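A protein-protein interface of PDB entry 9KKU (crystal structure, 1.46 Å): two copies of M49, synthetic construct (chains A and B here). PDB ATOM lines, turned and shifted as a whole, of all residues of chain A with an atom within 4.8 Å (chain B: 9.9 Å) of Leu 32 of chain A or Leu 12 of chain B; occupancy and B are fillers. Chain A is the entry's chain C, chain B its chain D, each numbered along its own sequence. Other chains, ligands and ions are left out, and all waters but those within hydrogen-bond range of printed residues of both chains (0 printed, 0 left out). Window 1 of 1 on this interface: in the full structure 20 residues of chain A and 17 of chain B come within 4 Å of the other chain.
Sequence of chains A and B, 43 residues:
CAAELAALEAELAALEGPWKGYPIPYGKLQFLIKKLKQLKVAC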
ATOM      1  N   LEU A   8     -17.203 -10.567 -23.758  1.00  0.00           N
ATOM      2  CA  LEU A   8     -16.024 -11.049 -24.493  1.00  0.00           C
ATOM      3  C   LEU A   8     -15.644 -12.426 -23.956  1.00  0.00           C
ATOM      4  O   LEU A   8     -15.419 -13.297 -24.789  1.00  0.00           O
ATOM      5  CB  LEU A   8     -14.893 -10.035 -24.347  1.00  0.00           C
ATOM      6  CG  LEU A   8     -15.286  -8.634 -24.845  1.00  0.00           C
ATOM      7  CD1 LEU A   8     -14.165  -7.614 -24.658  1.00  0.00           C
ATOM      8  CD2 LEU A   8     -15.751  -8.665 -26.301  1.00  0.00           C
ATOM      9  N   LEU A  12     -15.333 -15.532 -26.637  1.00  0.00           N
ATOM     10  CA  LEU A  12     -14.103 -16.348 -26.621  1.00  0.00           C
ATOM     11  C   LEU A  12     -14.430 -17.803 -26.276  1.00  0.00           C
ATOM     12  O   LEU A  12     -13.839 -18.702 -26.915  1.00  0.00           O
ATOM     13  CB  LEU A  12     -13.178 -15.749 -25.561  1.00  0.00           C
ATOM     14  CG  LEU A  12     -11.762 -16.298 -25.589  1.00  0.00           C
ATOM     15  CD1 LEU A  12     -11.177 -16.181 -26.988  1.00  0.00           C
ATOM     16  CD2 LEU A  12     -10.885 -15.599 -24.564  1.00  0.00           C
ATOM     17  N   TYR A  26      -6.127 -17.317 -36.052  1.00  0.00           N
ATOM     18  CA  TYR A  26      -5.898 -16.003 -35.367  1.00  0.00           C
ATOM     19  C   TYR A  26      -6.943 -14.965 -35.800  1.00  0.00           C
ATOM     20  O   TYR A  26      -7.335 -14.080 -34.957  1.00  0.00           O
ATOM     21  CB  TYR A  26      -4.493 -15.474 -35.656  1.00  0.00           C
ATOM     22  CG  TYR A  26      -4.108 -14.192 -34.952  1.00  0.00           C
ATOM     23  CD1 TYR A  26      -4.202 -14.084 -33.571  1.00  0.00           C
ATOM     24  CD2 TYR A  26      -3.603 -13.109 -35.665  1.00  0.00           C
ATOM     25  CE1 TYR A  26      -3.814 -12.930 -32.913  1.00  0.00           C
ATOM     26  CE2 TYR A  26      -3.217 -11.941 -35.020  1.00  0.00           C
ATOM     27  CZ  TYR A  26      -3.308 -11.860 -33.635  1.00  0.00           C
ATOM     28  OH  TYR A  26      -2.927 -10.711 -32.992  1.00  0.00           O
ATOM     29  N   LEU A  29      -9.839 -14.334 -33.489  1.00  0.00           N
ATOM     30  CA  LEU A  29      -9.620 -13.521 -32.247  1.00  0.00           C
ATOM     31  C   LEU A  29      -9.782 -12.013 -32.479  1.00  0.00           C
ATOM     32  O   LEU A  29      -9.648 -11.248 -31.471  1.00  0.00           O
ATOM     33  CB  LEU A  29      -8.229 -13.815 -31.683  1.00  0.00           C
ATOM     34  CG  LEU A  29      -8.073 -15.169 -30.996  1.00  0.00           C
ATOM     35  CD1 LEU A  29      -6.615 -15.403 -30.609  1.00  0.00           C
ATOM     36  CD2 LEU A  29      -8.965 -15.281 -29.772  1.00  0.00           C
ATOM     37  N   GLN A  30     -10.018 -11.574 -33.720  1.00  0.00           N
ATOM     38  CA  GLN A  30      -9.968 -10.127 -34.073  1.00  0.00           C
ATOM     39  C   GLN A  30     -11.034  -9.376 -33.264  1.00  0.00           C
ATOM     40  O   GLN A  30     -10.724  -8.262 -32.762  1.00  0.00           O
ATOM     41  CB  GLN A  30     -10.142  -9.925 -35.580  1.00  0.00           C
ATOM     42  CG  GLN A  30      -9.066 -10.615 -36.411  1.00  0.00           C
ATOM     43  CD  GLN A  30      -7.712 -10.604 -35.746  1.00  0.00           C
ATOM     44  OE1 GLN A  30      -7.128  -9.552 -35.490  1.00  0.00           O
ATOM     45  NE2 GLN A  30      -7.196 -11.786 -35.455  1.00  0.00           N
ATOM     46  N   PHE A  31     -12.238  -9.944 -33.144  1.00  0.00           N
ATOM     47  CA  PHE A  31     -13.357  -9.352 -32.354  1.00  0.00           C
ATOM     48  C   PHE A  31     -12.848  -8.895 -30.972  1.00  0.00           C
ATOM     49  O   PHE A  31     -13.243  -7.798 -30.493  1.00  0.00           O
ATOM     50  CB  PHE A  31     -14.510 -10.350 -32.199  1.00  0.00           C
ATOM     51  CG  PHE A  31     -14.286 -11.413 -31.153  1.00  0.00           C
ATOM     52  CD1 PHE A  31     -13.664 -12.612 -31.474  1.00  0.00           C
ATOM     53  CD2 PHE A  31     -14.685 -11.210 -29.838  1.00  0.00           C
ATOM     54  CE1 PHE A  31     -13.460 -13.581 -30.505  1.00  0.00           C
ATOM     55  CE2 PHE A  31     -14.467 -12.178 -28.867  1.00  0.00           C
ATOM     56  CZ  PHE A  31     -13.866 -13.366 -29.206  1.00  0.00           C
ATOM     57  N   LEU A  32     -12.003  -9.720 -30.336  1.00  0.00           N
ATOM     58  CA  LEU A  32     -11.486  -9.510 -28.954  1.00  0.00           C
ATOM     59  C   LEU A  32     -10.442  -8.389 -28.983  1.00  0.00           C
ATOM     60  O   LEU A  32     -10.475  -7.527 -28.085  1.00  0.00           O
ATOM     61  CB  LEU A  32     -10.907 -10.834 -28.427  1.00  0.00           C
ATOM     62  CG  LEU A  32     -10.418 -10.837 -26.977  1.00  0.00           C
ATOM     63  CD1 LEU A  32     -11.544 -10.500 -26.003  1.00  0.00           C
ATOM     64  CD2 LEU A  32      -9.806 -12.187 -26.613  1.00  0.00           C
ATOM     65  N   ILE A  33      -9.558  -8.383 -29.981  1.00  0.00           N
ATOM     66  CA  ILE A  33      -8.488  -7.348 -30.077  1.00  0.00           C
ATOM     67  C   ILE A  33      -9.187  -5.989 -30.141  1.00  0.00           C
ATOM     68  O   ILE A  33      -8.888  -5.099 -29.288  1.00  0.00           O
ATOM     69  CB  ILE A  33      -7.552  -7.600 -31.278  1.00  0.00           C
ATOM     70  CG1 ILE A  33      -6.811  -8.933 -31.125  1.00  0.00           C
ATOM     71  CG2 ILE A  33      -6.577  -6.447 -31.440  1.00  0.00           C
ATOM     72  CD1 ILE A  33      -6.231  -9.480 -32.409  1.00  0.00           C
ATOM     73  N   LYS A  34     -10.137  -5.877 -31.074  1.00  0.00           N
ATOM     74  CA  LYS A  34     -10.906  -4.635 -31.361  1.00  0.00           C
ATOM     75  C   LYS A  34     -11.637  -4.217 -30.080  1.00  0.00           C
ATOM     76  O   LYS A  34     -11.572  -3.024 -29.696  1.00  0.00           O
ATOM     77  CB  LYS A  34     -11.840  -4.887 -32.552  1.00  0.00           C
ATOM     78  CG  LYS A  34     -11.116  -5.157 -33.871  1.00  0.00           C
ATOM     79  CD  LYS A  34     -12.022  -5.297 -35.081  1.00  0.00           C
ATOM     80  CE  LYS A  34     -12.340  -6.733 -35.442  1.00  0.00           C
ATOM     81  NZ  LYS A  34     -13.595  -6.839 -36.226  1.00  0.00           N
ATOM     82  N   LYS A  35     -12.224  -5.185 -29.378  1.00  0.00           N
ATOM     83  CA  LYS A  35     -13.104  -4.890 -28.218  1.00  0.00           C
ATOM     84  C   LYS A  35     -12.253  -4.462 -27.009  1.00  0.00           C
ATOM     85  O   LYS A  35     -12.707  -3.562 -26.274  1.00  0.00           O
ATOM     86  CB  LYS A  35     -14.040  -6.072 -27.967  1.00  0.00           C
ATOM     87  CG  LYS A  35     -15.310  -6.057 -28.809  1.00  0.00           C
ATOM     88  CD  LYS A  35     -16.372  -5.107 -28.267  1.00  0.00           C
ATOM     89  CE  LYS A  35     -17.566  -4.945 -29.188  1.00  0.00           C
ATOM     90  NZ  LYS A  35     -17.852  -3.516 -29.470  1.00  0.00           N
ATOM     91  N   LEU A  36     -11.056  -5.023 -26.825  1.00  0.00           N
ATOM     92  CA  LEU A  36     -10.166  -4.660 -25.683  1.00  0.00           C
ATOM     93  C   LEU A  36      -9.516  -3.289 -25.909  1.00  0.00           C
ATOM     94  O   LEU A  36      -9.211  -2.610 -24.907  1.00  0.00           O
ATOM     95  CB  LEU A  36      -9.101  -5.744 -25.478  1.00  0.00           C
ATOM     96  CG  LEU A  36      -9.628  -7.127 -25.106  1.00  0.00           C
ATOM     97  CD1 LEU A  36      -8.487  -8.113 -25.002  1.00  0.00           C
ATOM     98  CD2 LEU A  36     -10.429  -7.104 -23.807  1.00  0.00           C
ATOM     99  N   GLU B   4      -3.917  -5.558 -16.234  1.00  0.00           N
ATOM    100  CA  GLU B   4      -4.360  -6.891 -16.733  1.00  0.00           C
ATOM    101  C   GLU B   4      -4.968  -6.727 -18.137  1.00  0.00           C
ATOM    102  O   GLU B   4      -4.744  -7.600 -18.983  1.00  0.00           O
ATOM    103  CB  GLU B   4      -5.383  -7.537 -15.785  1.00  0.00           C
ATOM    104  CG  GLU B   4      -4.804  -8.070 -14.475  1.00  0.00           C
ATOM    105  CD  GLU B   4      -5.000  -7.187 -13.250  1.00  0.00           C
ATOM    106  OE1 GLU B   4      -4.981  -5.934 -13.407  1.00  0.00           O
ATOM    107  OE2 GLU B   4      -5.144  -7.751 -12.132  1.00  0.00           O
ATOM    108  N   LEU B   5      -5.706  -5.644 -18.385  1.00  0.00           N
ATOM    109  CA  LEU B   5      -6.251  -5.349 -19.738  1.00  0.00           C
ATOM    110  C   LEU B   5      -5.088  -5.082 -20.694  1.00  0.00           C
ATOM    111  O   LEU B   5      -5.071  -5.671 -21.789  1.00  0.00           O
ATOM    112  CB  LEU B   5      -7.212  -4.159 -19.667  1.00  0.00           C
ATOM    113  CG  LEU B   5      -7.776  -3.687 -21.003  1.00  0.00           C
ATOM    114  CD1 LEU B   5      -8.565  -4.800 -21.673  1.00  0.00           C
ATOM    115  CD2 LEU B   5      -8.640  -2.451 -20.819  1.00  0.00           C
ATOM    116  N   ALA B   6      -4.156  -4.215 -20.311  1.00  0.00           N
ATOM    117  CA  ALA B   6      -2.988  -3.830 -21.140  1.00  0.00           C
ATOM    118  C   ALA B   6      -2.166  -5.082 -21.465  1.00  0.00           C
ATOM    119  O   ALA B   6      -1.741  -5.251 -22.620  1.00  0.00           O
ATOM    120  CB  ALA B   6      -2.169  -2.800 -20.398  1.00  0.00           C
ATOM    121  N   ALA B   7      -1.962  -5.931 -20.458  1.00  0.00           N
ATOM    122  CA  ALA B   7      -1.229  -7.217 -20.550  1.00  0.00           C
ATOM    123  C   ALA B   7      -1.905  -8.110 -21.597  1.00  0.00           C
ATOM    124  O   ALA B   7      -1.188  -8.624 -22.493  1.00  0.00           O
ATOM    125  CB  ALA B   7      -1.177  -7.877 -19.181  1.00  0.00           C
ATOM    126  N   LEU B   8      -3.235  -8.239 -21.546  1.00  0.00           N
ATOM    127  CA  LEU B   8      -3.952  -9.189 -22.431  1.00  0.00           C
ATOM    128  C   LEU B   8      -3.902  -8.624 -23.853  1.00  0.00           C
ATOM    129  O   LEU B   8      -3.684  -9.421 -24.806  1.00  0.00           O
ATOM    130  CB  LEU B   8      -5.387  -9.409 -21.941  1.00  0.00           C
ATOM    131  CG  LEU B   8      -6.150 -10.511 -22.678  1.00  0.00           C
ATOM    132  CD1 LEU B   8      -5.379 -11.831 -22.638  1.00  0.00           C
ATOM    133  CD2 LEU B   8      -7.534 -10.703 -22.095  1.00  0.00           C
ATOM    134  N   GLU B   9      -4.092  -7.313 -23.981  1.00  0.00           N
ATOM    135  CA  GLU B   9      -3.936  -6.567 -25.254  1.00  0.00           C
ATOM    136  C   GLU B   9      -2.610  -6.983 -25.894  1.00  0.00           C
ATOM    137  O   GLU B   9      -2.629  -7.452 -27.049  1.00  0.00           O
ATOM    138  CB  GLU B   9      -4.021  -5.060 -25.007  1.00  0.00           C
ATOM    139  CG  GLU B   9      -3.474  -4.212 -26.147  1.00  0.00           C
ATOM    140  CD  GLU B   9      -4.078  -4.478 -27.515  1.00  0.00           C
ATOM    141  OE1 GLU B   9      -5.231  -4.063 -27.743  1.00  0.00           O
ATOM    142  OE2 GLU B   9      -3.388  -5.098 -28.353  1.00  0.00           O
ATOM    143  N   ALA B  10      -1.504  -6.818 -25.165  1.00  0.00           N
ATOM    144  CA  ALA B  10      -0.125  -7.021 -25.674  1.00  0.00           C
ATOM    145  C   ALA B  10       0.103  -8.502 -26.000  1.00  0.00           C
ATOM    146  O   ALA B  10       0.842  -8.782 -26.958  1.00  0.00           O
ATOM    147  CB  ALA B  10       0.878  -6.506 -24.675  1.00  0.00           C
ATOM    148  N   GLU B  11      -0.539  -9.413 -25.267  1.00  0.00           N
ATOM    149  CA  GLU B  11      -0.444 -10.881 -25.510  1.00  0.00           C
ATOM    150  C   GLU B  11      -1.188 -11.248 -26.798  1.00  0.00           C
ATOM    151  O   GLU B  11      -0.619 -11.939 -27.637  1.00  0.00           O
ATOM    152  CB  GLU B  11      -0.982 -11.677 -24.323  1.00  0.00           C
ATOM    153  CG  GLU B  11       0.017 -11.808 -23.183  1.00  0.00           C
ATOM    154  CD  GLU B  11      -0.431 -12.750 -22.075  1.00  0.00           C
ATOM    155  OE1 GLU B  11      -1.668 -12.846 -21.834  1.00  0.00           O
ATOM    156  OE2 GLU B  11       0.454 -13.391 -21.455  1.00  0.00           O
ATOM    157  N   LEU B  12      -2.413 -10.758 -26.962  1.00  0.00           N
ATOM    158  CA  LEU B  12      -3.198 -10.959 -28.193  1.00  0.00           C
ATOM    159  C   LEU B  12      -2.474 -10.362 -29.400  1.00  0.00           C
ATOM    160  O   LEU B  12      -2.464 -11.025 -30.464  1.00  0.00           O
ATOM    161  CB  LEU B  12      -4.558 -10.295 -27.997  1.00  0.00           C
ATOM    162  CG  LEU B  12      -5.542 -11.085 -27.150  1.00  0.00           C
ATOM    163  CD1 LEU B  12      -6.775 -10.234 -26.850  1.00  0.00           C
ATOM    164  CD2 LEU B  12      -5.952 -12.369 -27.845  1.00  0.00           C
ATOM    165  N   ALA B  13      -1.960  -9.140 -29.292  1.00  0.00           N
ATOM    166  CA  ALA B  13      -1.280  -8.450 -30.414  1.00  0.00           C
ATOM    167  C   ALA B  13      -0.089  -9.302 -30.878  1.00  0.00           C
ATOM    168  O   ALA B  13       0.094  -9.438 -32.125  1.00  0.00           O
ATOM    169  CB  ALA B  13      -0.832  -7.065 -29.994  1.00  0.00           C
ATOM    170  N   ALA B  14       0.670  -9.849 -29.919  1.00  0.00           N
ATOM    171  CA  ALA B  14       1.952 -10.562 -30.131  1.00  0.00           C
ATOM    172  C   ALA B  14       1.717 -12.069 -30.313  1.00  0.00           C
ATOM    173  O   ALA B  14       2.714 -12.792 -30.497  1.00  0.00           O
ATOM    174  CB  ALA B  14       2.876 -10.294 -28.963  1.00  0.00           C
ATOM    175  N   LEU B  15       0.455 -12.516 -30.271  1.00  0.00           N
ATOM    176  CA  LEU B  15       0.072 -13.926 -30.031  1.00  0.00           C
ATOM    177  C   LEU B  15       0.708 -14.830 -31.095  1.00  0.00           C
ATOM    178  O   LEU B  15       1.167 -15.926 -30.719  1.00  0.00           O
ATOM    179  CB  LEU B  15      -1.450 -14.065 -30.043  1.00  0.00           C
ATOM    180  CG  LEU B  15      -1.982 -15.383 -29.488  1.00  0.00           C
ATOM    181  CD1 LEU B  15      -1.533 -15.592 -28.044  1.00  0.00           C
ATOM    182  CD2 LEU B  15      -3.499 -15.436 -29.605  1.00  0.00           C
ATOM    183  N   GLU B  16       0.740 -14.395 -32.357  1.00  0.00           N
ATOM    184  CA  GLU B  16       1.324 -15.204 -33.453  1.00  0.00           C
ATOM    185  C   GLU B  16       2.824 -15.432 -33.170  1.00  0.00           C
ATOM    186  O   GLU B  16       3.341 -16.503 -33.564  1.00  0.00           O
ATOM    187  CB  GLU B  16       1.017 -14.587 -34.828  1.00  0.00           C
ATOM    188  CG  GLU B  16       1.717 -13.262 -35.129  1.00  0.00           C
ATOM    189  CD  GLU B  16       0.885 -11.999 -34.923  1.00  0.00           C
ATOM    190  OE1 GLU B  16       0.563 -11.692 -33.741  1.00  0.00           O
ATOM    191  OE2 GLU B  16       0.558 -11.322 -35.944  1.00  0.00           O
ATOM    192  N   GLY B  17       3.489 -14.521 -32.446  1.00  0.00           N
ATOM    193  CA  GLY B  17       4.953 -14.384 -32.486  1.00  0.00           C
ATOM    194  C   GLY B  17       5.424 -14.299 -33.933  1.00  0.00           C
ATOM    195  O   GLY B  17       4.861 -13.556 -34.741  1.00  0.00           O
ATOM    196  N   ILE B  24      -3.535 -20.802 -33.595  1.00  0.00           N
ATOM    197  CA  ILE B  24      -3.204 -20.582 -32.185  1.00  0.00           C
ATOM    198  C   ILE B  24      -3.499 -21.876 -31.447  1.00  0.00           C
ATOM    199  O   ILE B  24      -4.634 -22.333 -31.441  1.00  0.00           O
ATOM    200  CB  ILE B  24      -4.104 -19.438 -31.686  1.00  0.00           C
ATOM    201  CG1 ILE B  24      -3.914 -18.163 -32.516  1.00  0.00           C
ATOM    202  CG2 ILE B  24      -3.894 -19.250 -30.210  1.00  0.00           C
ATOM    203  CD1 ILE B  24      -2.487 -17.677 -32.542  1.00  0.00           C
ATOM    204  N   LYS B  28      -3.023 -22.238 -25.794  1.00  0.00           N
ATOM    205  CA  LYS B  28      -2.954 -20.757 -25.777  1.00  0.00           C
ATOM    206  C   LYS B  28      -4.374 -20.172 -25.685  1.00  0.00           C
ATOM    207  O   LYS B  28      -4.565 -19.230 -24.923  1.00  0.00           O
ATOM    208  CB  LYS B  28      -2.189 -20.255 -27.008  1.00  0.00           C
ATOM    209  CG  LYS B  28      -0.678 -20.441 -26.938  1.00  0.00           C
ATOM    210  CD  LYS B  28       0.123 -19.338 -27.624  1.00  0.00           C
ATOM    211  CE  LYS B  28       1.595 -19.655 -27.769  1.00  0.00           C
ATOM    212  NZ  LYS B  28       1.908 -20.132 -29.136  1.00  0.00           N
ATOM    213  N   LEU B  29      -5.352 -20.716 -26.415  1.00  0.00           N
ATOM    214  CA  LEU B  29      -6.774 -20.266 -26.309  1.00  0.00           C
ATOM    215  C   LEU B  29      -7.249 -20.443 -24.848  1.00  0.00           C
ATOM    216  O   LEU B  29      -7.872 -19.523 -24.285  1.00  0.00           O
ATOM    217  CB  LEU B  29      -7.609 -21.098 -27.295  1.00  0.00           C
ATOM    218  CG  LEU B  29      -9.126 -20.981 -27.144  1.00  0.00           C
ATOM    219  CD1 LEU B  29      -9.615 -19.562 -27.396  1.00  0.00           C
ATOM    220  CD2 LEU B  29      -9.846 -21.952 -28.052  1.00  0.00           C
ATOM    221  N   PHE B  31      -5.420 -20.537 -22.164  1.00  0.00           N
ATOM    222  CA  PHE B  31      -4.633 -19.587 -21.339  1.00  0.00           C
ATOM    223  C   PHE B  31      -5.301 -18.210 -21.438  1.00  0.00           C
ATOM    224  O   PHE B  31      -5.552 -17.585 -20.396  1.00  0.00           O
ATOM    225  CB  PHE B  31      -3.168 -19.549 -21.774  1.00  0.00           C
ATOM    226  CG  PHE B  31      -2.423 -18.351 -21.243  1.00  0.00           C
ATOM    227  CD1 PHE B  31      -1.979 -18.322 -19.929  1.00  0.00           C
ATOM    228  CD2 PHE B  31      -2.213 -17.237 -22.045  1.00  0.00           C
ATOM    229  CE1 PHE B  31      -1.317 -17.210 -19.433  1.00  0.00           C
ATOM    230  CE2 PHE B  31      -1.549 -16.126 -21.549  1.00  0.00           C
ATOM    231  CZ  PHE B  31      -1.102 -16.115 -20.244  1.00  0.00           C
ATOM    232  N   LEU B  32      -5.607 -17.778 -22.670  1.00  0.00           N
ATOM    233  CA  LEU B  32      -6.356 -16.525 -22.952  1.00  0.00           C
ATOM    234  C   LEU B  32      -7.696 -16.534 -22.215  1.00  0.00           C
ATOM    235  O   LEU B  32      -8.037 -15.489 -21.649  1.00  0.00           O
ATOM    236  CB  LEU B  32      -6.590 -16.389 -24.463  1.00  0.00           C
ATOM    237  CG  LEU B  32      -5.396 -15.881 -25.266  1.00  0.00           C
ATOM    238  CD1 LEU B  32      -5.681 -15.950 -26.754  1.00  0.00           C
ATOM    239  CD2 LEU B  32      -5.047 -14.458 -24.845  1.00  0.00           C
ATOM    240  N   ILE B  33      -8.452 -17.636 -22.272  1.00  0.00           N
ATOM    241  CA  ILE B  33      -9.794 -17.746 -21.625  1.00  0.00           C
ATOM    242  C   ILE B  33      -9.600 -17.522 -20.120  1.00  0.00           C
ATOM    243  O   ILE B  33     -10.377 -16.756 -19.537  1.00  0.00           O
ATOM    244  CB  ILE B  33     -10.484 -19.090 -21.954  1.00  0.00           C
ATOM    245  CG1 ILE B  33     -10.968 -19.130 -23.411  1.00  0.00           C
ATOM    246  CG2 ILE B  33     -11.625 -19.393 -20.983  1.00  0.00           C
ATOM    247  CD1 ILE B  33     -11.652 -20.426 -23.830  1.00  0.00           C
ATOM    248  N   LYS B  34      -8.581 -18.164 -19.545  1.00  0.00           N
ATOM    249  CA  LYS B  34      -8.228 -18.067 -18.108  1.00  0.00           C
ATOM    250  C   LYS B  34      -7.863 -16.613 -17.792  1.00  0.00           C
ATOM    251  O   LYS B  34      -8.441 -16.045 -16.856  1.00  0.00           O
ATOM    252  CB  LYS B  34      -7.081 -19.028 -17.794  1.00  0.00           C
ATOM    253  CG  LYS B  34      -6.568 -18.978 -16.362  1.00  0.00           C
ATOM    254  CD  LYS B  34      -6.198 -20.340 -15.800  1.00  0.00           C
ATOM    255  CE  LYS B  34      -5.941 -20.312 -14.308  1.00  0.00           C
ATOM    256  NZ  LYS B  34      -5.375 -21.593 -13.820  1.00  0.00           N
ATOM    257  N   LYS B  35      -6.969 -16.022 -18.585  1.00  0.00           N
ATOM    258  CA  LYS B  35      -6.538 -14.611 -18.421  1.00  0.00           C
ATOM    259  C   LYS B  35      -7.762 -13.685 -18.514  1.00  0.00           C
ATOM    260  O   LYS B  35      -7.905 -12.783 -17.657  1.00  0.00           O
ATOM    261  CB  LYS B  35      -5.471 -14.303 -19.477  1.00  0.00           C
ATOM    262  CG  LYS B  35      -4.144 -15.026 -19.275  1.00  0.00           C
ATOM    263  CD  LYS B  35      -3.477 -14.752 -17.939  1.00  0.00           C
ATOM    264  CE  LYS B  35      -3.267 -13.274 -17.701  1.00  0.00           C
ATOM    265  NZ  LYS B  35      -2.311 -13.033 -16.596  1.00  0.00           N
ATOM    266  N   LEU B  36      -8.647 -13.904 -19.493  1.00  0.00           N
ATOM    267  CA  LEU B  36      -9.832 -13.028 -19.698  1.00  0.00           C
ATOM    268  C   LEU B  36     -10.812 -13.172 -18.522  1.00  0.00           C
ATOM    269  O   LEU B  36     -11.433 -12.142 -18.116  1.00  0.00           O
ATOM    270  CB  LEU B  36     -10.508 -13.401 -21.025  1.00  0.00           C
ATOM    271  CG  LEU B  36     -11.703 -12.532 -21.411  1.00  0.00           C
ATOM    272  CD1 LEU B  36     -11.344 -11.051 -21.335  1.00  0.00           C
ATOM    273  CD2 LEU B  36     -12.216 -12.902 -22.809  1.00  0.00           C
ATOM    274  N   LYS B  37     -10.967 -14.389 -18.003  1.00  0.00           N
ATOM    275  CA  LYS B  37     -11.824 -14.700 -16.828  1.00  0.00           C
ATOM    276  C   LYS B  37     -11.232 -14.024 -15.585  1.00  0.00           C
ATOM    277  O   LYS B  37     -12.000 -13.381 -14.866  1.00  0.00           O
ATOM    278  CB  LYS B  37     -11.909 -16.211 -16.607  1.00  0.00           C
ATOM    279  CG  LYS B  37     -12.830 -16.661 -15.484  1.00  0.00           C
ATOM    280  CD  LYS B  37     -12.675 -18.138 -15.203  1.00  0.00           C
ATOM    281  CE  LYS B  37     -13.284 -18.572 -13.889  1.00  0.00           C
ATOM    282  NZ  LYS B  37     -14.709 -18.942 -14.052  1.00  0.00           N
ATOM    283  N   LEU B  39      -9.394 -11.491 -15.653  1.00  0.00           N
ATOM    284  CA  LEU B  39      -9.505 -10.032 -15.938  1.00  0.00           C
ATOM    285  C   LEU B  39     -10.935  -9.590 -15.612  1.00  0.00           C
ATOM    286  O   LEU B  39     -11.076  -8.472 -15.094  1.00  0.00           O
ATOM    287  CB  LEU B  39      -9.129  -9.696 -17.387  1.00  0.00           C
ATOM    288  CG  LEU B  39      -9.443  -8.262 -17.824  1.00  0.00           C
ATOM    289  CD1 LEU B  39      -8.659  -7.249 -16.998  1.00  0.00           C
ATOM    290  CD2 LEU B  39      -9.194  -8.059 -19.318  1.00  0.00           C
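Printed residues of chain B that touch a printed residue of chain A: Leu 5, Leu 12, Ala 13, Leu 15, Glu 16, Leu 29, Ile 33 and Leu 36. Hydrophobic or aromatic side chains of chain B within 4 Å of the printed part of chain A: Leu 5, Leu 12, Leu 15, Leu 29, Ile 33 and Leu 36. Among the printed residues, 12 pairs touch across the chains. Among the printed residues, no Asp or Glu carboxylate lies within 4 Å of a Lys or Arg side-chain nitrogen of the other chain.
The side-chain hydroxyl of Tyr 26 of chain A is in hydrogen-bond range of the backbone carbonyl oxygen of Leu 12 of chain B (2.6 Å). The side-chain hydroxyl (OH) of Tyr 26 of chain A is in hydrogen-bond range of the backbone carbonyl oxygen (O) of Ala 13 of chain B (3.4 Å).
Leu 8 of chain A touches Leu 36 of chain B, but with the chains exchanged Leu 36 of chain A does not touch Leu 8 of chain B (4.01 Å). Leu 12 of chain A touches Leu 29 of chain B, but with the chains exchanged Leu 29 of chain A does not touch Leu 12 of chain B (4.2 Å). Leu 12 of chain A touches Ile 33 of chain B, but with the chains exchanged Ile 33 of chain A does not touch Leu 12 of chain B (4.1 Å). Leu 32 of chain A touches Leu 12 of chain B, but with the chains exchanged Leu 12 of chain A does not touch Leu 32 of chain B (4.1 Å). 9 positions are printed for both chains. Of the 12 pairs that touch across the chains among the printed residues, 2 have their exchanged pair printed and touching as well.
Leu 8 of chain A touches Leu 36 of chain B (C to CD2, 3.6 Å). CD1 of Leu 12 of chain A touches CD1 of Leu 29 of chain B, 3.7 Å away. Leu 12 of chain A touches Ile 33 of chain B. CD2 of Leu 36 of chain B touches CD2 of Leu 12 of chain A, 3.5 Å away. CE1 of Tyr 26 of chain A touches CB of Leu 15 of chain B, at 3.9 Å. Tyr 26 of chain A touches Glu 16 of chain B. Leu 29 of chain A touches Leu 15 of chain B (CD1 to CD2, 3.3 Å). Leu 12 of chain B touches Leu 32 of chain A. CD2 of Leu 36 of chain A touches CD1 of Leu 5 of chain B, at 3.7 Å. Leu 36 of chain A touches Leu 12 of chain B (CD1 to CD1, 3.3 Å).
No residue of chain B comes within 4 Å of Phe 31 of chain A. Ile 33 of chain A touches none of the printed residues of chain B. Printed residues of chain A within 4 Å of Leu 5 of chain B: Leu 36 (3.7 Å). Leu 12 of chain B touches just these residues of chain A: Tyr 26, Leu 32 and Leu 36. Of the printed residues of chain A, Ala 13 of chain B touches Tyr 26 (3.4 Å). Printed residues of chain A within 4 Å of Glu 16 of chain B: Tyr 26 (3.7 Å). Leu 32 of chain B touches none of the printed residues of chain A. Of the printed residues of chain A, Leu 36 of chain B touches Leu 8 and Leu 12.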
